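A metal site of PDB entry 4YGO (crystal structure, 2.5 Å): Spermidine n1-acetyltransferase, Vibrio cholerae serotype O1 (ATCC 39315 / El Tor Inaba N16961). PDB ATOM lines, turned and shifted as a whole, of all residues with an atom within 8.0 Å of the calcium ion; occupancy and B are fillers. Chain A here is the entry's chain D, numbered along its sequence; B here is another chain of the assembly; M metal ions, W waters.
The side-chain hydroxyl of Tyr 78 of chain B sits at hydrogen-bond distance from the backbone carbonyl oxygen of Asn 53 of chain B (2.7 Å). OG of Ser 38 is in hydrogen-bond range of N of Glu 41 (3.3 Å). OE1 of Glu 41 lies close to ND1 of His 51 of chain B.
The nearest printed residue that does not touch the calcium ion is Tyr 36 (4.2 Å).
The calcium ion is bound by OE1 of Glu 41, at 2.3 Å. O of Pro 35 is bound to the calcium ion (2.3 Å). Water W1 binds the calcium ion. The calcium ion is bound by OD1 of Asn 53 of chain B, at 2.5 Å. The calcium ion is bound by the side-chain carboxylate (OE2) of Glu 41, at 2.8 Å. The calcium ion is bound by OE1 of Glu 34, 2.8 Å away.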
ATOM      1  N   MET A  28      -0.076   9.319 -17.872  1.00  0.00           N
ATOM      2  CA  MET A  28       0.789  10.397 -17.580  1.00  0.00           C
ATOM      3  C   MET A  28       1.946  10.341 -18.508  1.00  0.00           C
ATOM      4  O   MET A  28       2.460   9.287 -18.773  1.00  0.00           O
ATOM      5  CB  MET A  28       1.352  10.276 -16.185  1.00  0.00           C
ATOM      6  CG  MET A  28       2.274  11.449 -15.795  1.00  0.00           C
ATOM      7  SD  MET A  28       1.361  13.027 -15.783  1.00  0.00           S
ATOM      8  CE  MET A  28       0.434  12.707 -14.297  1.00  0.00           C
ATOM      9  N   SER A  29       2.405  11.501 -18.969  1.00  0.00           N
ATOM     10  CA  SER A  29       3.490  11.538 -19.905  1.00  0.00           C
ATOM     11  C   SER A  29       4.624  12.300 -19.327  1.00  0.00           C
ATOM     12  O   SER A  29       4.469  13.066 -18.354  1.00  0.00           O
ATOM     13  CB  SER A  29       3.045  12.231 -21.137  1.00  0.00           C
ATOM     14  OG  SER A  29       2.859  13.609 -20.815  1.00  0.00           O
ATOM     15  N   GLU A  34      10.494  14.249 -16.415  1.00  0.00           N
ATOM     16  CA  GLU A  34       9.595  15.209 -15.693  1.00  0.00           C
ATOM     17  C   GLU A  34       8.195  14.897 -16.222  1.00  0.00           C
ATOM     18  O   GLU A  34       8.040  14.794 -17.452  1.00  0.00           O
ATOM     19  CB  GLU A  34       9.942  16.663 -16.044  1.00  0.00           C
ATOM     20  CG  GLU A  34       9.991  17.727 -14.928  1.00  0.00           C
ATOM     21  CD  GLU A  34       9.013  17.599 -13.753  1.00  0.00           C
ATOM     22  OE1 GLU A  34       7.946  18.287 -13.666  1.00  0.00           O
ATOM     23  OE2 GLU A  34       9.399  16.836 -12.853  1.00  0.00           O
ATOM     24  N   PRO A  35       7.190  14.707 -15.328  1.00  0.00           N
ATOM     25  CA  PRO A  35       5.831  14.556 -15.814  1.00  0.00           C
ATOM     26  C   PRO A  35       5.227  15.894 -16.186  1.00  0.00           C
ATOM     27  O   PRO A  35       5.442  16.918 -15.502  1.00  0.00           O
ATOM     28  CB  PRO A  35       5.087  13.947 -14.621  1.00  0.00           C
ATOM     29  CG  PRO A  35       5.882  14.364 -13.426  1.00  0.00           C
ATOM     30  CD  PRO A  35       7.298  14.335 -13.903  1.00  0.00           C
ATOM     31  N   TYR A  36       4.475  15.893 -17.271  1.00  0.00           N
ATOM     32  CA  TYR A  36       3.755  17.108 -17.644  1.00  0.00           C
ATOM     33  C   TYR A  36       2.312  16.771 -18.071  1.00  0.00           C
ATOM     34  O   TYR A  36       2.029  15.671 -18.554  1.00  0.00           O
ATOM     35  CB  TYR A  36       4.476  17.838 -18.780  1.00  0.00           C
ATOM     36  CG  TYR A  36       4.382  17.094 -20.107  1.00  0.00           C
ATOM     37  CD1 TYR A  36       5.287  16.075 -20.431  1.00  0.00           C
ATOM     38  CD2 TYR A  36       3.348  17.394 -21.026  1.00  0.00           C
ATOM     39  CE1 TYR A  36       5.193  15.415 -21.651  1.00  0.00           C
ATOM     40  CE2 TYR A  36       3.220  16.714 -22.222  1.00  0.00           C
ATOM     41  CZ  TYR A  36       4.126  15.725 -22.529  1.00  0.00           C
ATOM     42  OH  TYR A  36       3.979  15.056 -23.730  1.00  0.00           O
ATOM     43  N   GLU A  37       1.428  17.742 -17.928  1.00  0.00           N
ATOM     44  CA  GLU A  37       0.088  17.636 -18.468  1.00  0.00           C
ATOM     45  C   GLU A  37      -0.235  18.767 -19.440  1.00  0.00           C
ATOM     46  O   GLU A  37      -0.849  18.501 -20.457  1.00  0.00           O
ATOM     47  CB  GLU A  37      -0.938  17.567 -17.358  1.00  0.00           C
ATOM     48  CG  GLU A  37      -0.736  16.366 -16.465  1.00  0.00           C
ATOM     49  CD  GLU A  37      -1.346  16.526 -15.073  1.00  0.00           C
ATOM     50  OE1 GLU A  37      -1.546  15.480 -14.467  1.00  0.00           O
ATOM     51  OE2 GLU A  37      -1.608  17.654 -14.571  1.00  0.00           O
ATOM     52  N   SER A  38       0.127  20.017 -19.137  1.00  0.00           N
ATOM     53  CA  SER A  38      -0.230  21.078 -20.089  1.00  0.00           C
ATOM     54  C   SER A  38       0.802  21.237 -21.138  1.00  0.00           C
ATOM     55  O   SER A  38       2.003  21.086 -20.905  1.00  0.00           O
ATOM     56  CB  SER A  38      -0.397  22.418 -19.431  1.00  0.00           C
ATOM     57  OG  SER A  38       0.812  22.873 -18.918  1.00  0.00           O
ATOM     58  N   GLU A  41       3.822  23.435 -20.126  1.00  0.00           N
ATOM     59  CA  GLU A  41       4.923  22.754 -19.441  1.00  0.00           C
ATOM     60  C   GLU A  41       5.759  21.942 -20.444  1.00  0.00           C
ATOM     61  O   GLU A  41       6.995  21.899 -20.340  1.00  0.00           O
ATOM     62  CB  GLU A  41       4.389  21.880 -18.299  1.00  0.00           C
ATOM     63  CG  GLU A  41       5.521  21.439 -17.386  1.00  0.00           C
ATOM     64  CD  GLU A  41       5.152  20.501 -16.259  1.00  0.00           C
ATOM     65  OE1 GLU A  41       6.086  20.306 -15.445  1.00  0.00           O
ATOM     66  OE2 GLU A  41       3.971  20.037 -16.176  1.00  0.00           O
ATOM     67  N   LEU A  42       5.082  21.307 -21.389  1.00  0.00           N
ATOM     68  CA  LEU A  42       5.739  20.616 -22.452  1.00  0.00           C
ATOM     69  C   LEU A  42       6.686  21.559 -23.209  1.00  0.00           C
ATOM     70  O   LEU A  42       7.841  21.239 -23.471  1.00  0.00           O
ATOM     71  CB  LEU A  42       4.706  19.979 -23.394  1.00  0.00           C
ATOM     72  CG  LEU A  42       5.271  19.283 -24.659  1.00  0.00           C
ATOM     73  CD1 LEU A  42       6.245  18.210 -24.291  1.00  0.00           C
ATOM     74  CD2 LEU A  42       4.198  18.753 -25.622  1.00  0.00           C
ATOM     75  N   LEU A  45       9.777  22.544 -20.879  1.00  0.00           N
ATOM     76  CA  LEU A  45      10.650  21.376 -20.890  1.00  0.00           C
ATOM     77  C   LEU A  45      11.450  21.160 -22.223  1.00  0.00           C
ATOM     78  O   LEU A  45      12.689  20.833 -22.226  1.00  0.00           O
ATOM     79  CB  LEU A  45       9.802  20.148 -20.621  1.00  0.00           C
ATOM     80  CG  LEU A  45       9.660  19.503 -19.242  1.00  0.00           C
ATOM     81  CD1 LEU A  45      10.370  20.231 -18.139  1.00  0.00           C
ATOM     82  CD2 LEU A  45       8.201  19.262 -18.954  1.00  0.00           C
ATOM     83  N   HIS B  49       5.446  28.725 -11.357  1.00  0.00           N
ATOM     84  CA  HIS B  49       5.156  27.423 -10.767  1.00  0.00           C
ATOM     85  C   HIS B  49       4.856  26.358 -11.821  1.00  0.00           C
ATOM     86  O   HIS B  49       4.418  25.239 -11.498  1.00  0.00           O
ATOM     87  CB  HIS B  49       4.012  27.531  -9.732  1.00  0.00           C
ATOM     88  CG  HIS B  49       4.376  28.230  -8.458  1.00  0.00           C
ATOM     89  ND1 HIS B  49       4.956  27.585  -7.382  1.00  0.00           N
ATOM     90  CD2 HIS B  49       4.200  29.506  -8.054  1.00  0.00           C
ATOM     91  CE1 HIS B  49       5.155  28.433  -6.398  1.00  0.00           C
ATOM     92  NE2 HIS B  49       4.713  29.614  -6.774  1.00  0.00           N
ATOM     93  N   ILE B  50       5.195  26.621 -13.064  1.00  0.00           N
ATOM     94  CA  ILE B  50       4.946  25.699 -14.182  1.00  0.00           C
ATOM     95  C   ILE B  50       5.456  24.288 -13.919  1.00  0.00           C
ATOM     96  O   ILE B  50       4.845  23.343 -14.396  1.00  0.00           O
ATOM     97  CB  ILE B  50       5.607  26.236 -15.499  1.00  0.00           C
ATOM     98  CG1 ILE B  50       5.005  25.573 -16.719  1.00  0.00           C
ATOM     99  CG2 ILE B  50       7.124  26.054 -15.526  1.00  0.00           C
ATOM    100  CD1 ILE B  50       3.658  26.194 -17.094  1.00  0.00           C
ATOM    101  N   HIS B  51       6.568  24.108 -13.198  1.00  0.00           N
ATOM    102  CA  HIS B  51       7.108  22.772 -12.985  1.00  0.00           C
ATOM    103  C   HIS B  51       6.811  22.228 -11.608  1.00  0.00           C
ATOM    104  O   HIS B  51       7.306  21.162 -11.305  1.00  0.00           O
ATOM    105  CB  HIS B  51       8.643  22.737 -13.172  1.00  0.00           C
ATOM    106  CG  HIS B  51       9.103  23.169 -14.527  1.00  0.00           C
ATOM    107  ND1 HIS B  51       8.718  22.522 -15.684  1.00  0.00           N
ATOM    108  CD2 HIS B  51       9.915  24.177 -14.898  1.00  0.00           C
ATOM    109  CE1 HIS B  51       9.258  23.129 -16.725  1.00  0.00           C
ATOM    110  NE2 HIS B  51      10.007  24.135 -16.280  1.00  0.00           N
ATOM    111  N   ASP B  52       6.010  22.936 -10.817  1.00  0.00           N
ATOM    112  CA  ASP B  52       5.581  22.484  -9.534  1.00  0.00           C
ATOM    113  C   ASP B  52       4.405  21.499  -9.671  1.00  0.00           C
ATOM    114  O   ASP B  52       3.300  21.850 -10.159  1.00  0.00           O
ATOM    115  CB  ASP B  52       5.173  23.694  -8.696  1.00  0.00           C
ATOM    116  CG  ASP B  52       5.158  23.432  -7.179  1.00  0.00           C
ATOM    117  OD1 ASP B  52       5.107  22.271  -6.705  1.00  0.00           O
ATOM    118  OD2 ASP B  52       5.234  24.455  -6.438  1.00  0.00           O
ATOM    119  N   ASN B  53       4.628  20.287  -9.218  1.00  0.00           N
ATOM    120  CA  ASN B  53       3.590  19.213  -9.200  1.00  0.00           C
ATOM    121  C   ASN B  53       2.657  19.152  -7.994  1.00  0.00           C
ATOM    122  O   ASN B  53       1.873  18.217  -7.874  1.00  0.00           O
ATOM    123  CB  ASN B  53       4.304  17.848  -9.370  1.00  0.00           C
ATOM    124  CG  ASN B  53       5.026  17.776 -10.724  1.00  0.00           C
ATOM    125  OD1 ASN B  53       4.387  17.914 -11.767  1.00  0.00           O
ATOM    126  ND2 ASN B  53       6.331  17.569 -10.721  1.00  0.00           N
ATOM    127  N   ALA B  54       2.755  20.087  -7.060  1.00  0.00           N
ATOM    128  CA  ALA B  54       1.891  20.018  -5.855  1.00  0.00           C
ATOM    129  C   ALA B  54       0.453  20.437  -6.156  1.00  0.00           C
ATOM    130  O   ALA B  54      -0.414  20.204  -5.345  1.00  0.00           O
ATOM    131  CB  ALA B  54       2.461  20.815  -4.702  1.00  0.00           C
ATOM    132  N   GLU B  55       0.198  21.039  -7.324  1.00  0.00           N
ATOM    133  CA  GLU B  55      -1.176  21.393  -7.735  1.00  0.00           C
ATOM    134  C   GLU B  55      -1.285  21.128  -9.216  1.00  0.00           C
ATOM    135  O   GLU B  55      -0.325  21.224  -9.958  1.00  0.00           O
ATOM    136  CB  GLU B  55      -1.504  22.876  -7.377  1.00  0.00           C
ATOM    137  CG  GLU B  55      -1.134  23.253  -5.942  1.00  0.00           C
ATOM    138  CD  GLU B  55      -1.533  24.682  -5.513  1.00  0.00           C
ATOM    139  OE1 GLU B  55      -1.553  24.954  -4.265  1.00  0.00           O
ATOM    140  OE2 GLU B  55      -1.839  25.503  -6.413  1.00  0.00           O
ATOM    141  N   ARG B  56      -2.469  20.732  -9.648  1.00  0.00           N
ATOM    142  CA  ARG B  56      -2.718  20.324 -11.014  1.00  0.00           C
ATOM    143  C   ARG B  56      -4.139  20.791 -11.283  1.00  0.00           C
ATOM    144  O   ARG B  56      -4.977  20.762 -10.398  1.00  0.00           O
ATOM    145  CB  ARG B  56      -2.589  18.807 -11.153  1.00  0.00           C
ATOM    146  CG  ARG B  56      -1.179  18.285 -10.916  1.00  0.00           C
ATOM    147  CD  ARG B  56      -1.072  16.799 -11.232  1.00  0.00           C
ATOM    148  NE  ARG B  56       0.125  16.070 -10.732  1.00  0.00           N
ATOM    149  CZ  ARG B  56       1.194  15.683 -11.446  1.00  0.00           C
ATOM    150  NH1 ARG B  56       1.326  15.947 -12.759  1.00  0.00           N
ATOM    151  NH2 ARG B  56       2.166  15.024 -10.837  1.00  0.00           N
ATOM    152  N   TYR B  78       3.009  13.118  -2.420  1.00  0.00           N
ATOM    153  CA  TYR B  78       3.258  11.879  -3.096  1.00  0.00           C
ATOM    154  C   TYR B  78       3.889  10.795  -2.200  1.00  0.00           C
ATOM    155  O   TYR B  78       4.309   9.776  -2.735  1.00  0.00           O
ATOM    156  CB  TYR B  78       4.175  12.154  -4.289  1.00  0.00           C
ATOM    157  CG  TYR B  78       3.570  13.056  -5.311  1.00  0.00           C
ATOM    158  CD1 TYR B  78       2.798  12.529  -6.342  1.00  0.00           C
ATOM    159  CD2 TYR B  78       3.802  14.463  -5.279  1.00  0.00           C
ATOM    160  CE1 TYR B  78       2.227  13.355  -7.304  1.00  0.00           C
ATOM    161  CE2 TYR B  78       3.236  15.297  -6.244  1.00  0.00           C
ATOM    162  CZ  TYR B  78       2.441  14.751  -7.265  1.00  0.00           C
ATOM    163  OH  TYR B  78       1.831  15.553  -8.264  1.00  0.00           O
HETATM  164 CA    CA M   1       5.177  18.711 -14.035  1.00  0.00          CA
HETATM  165  O   HOH W   1       2.938  17.876 -14.206  1.00  0.00           O
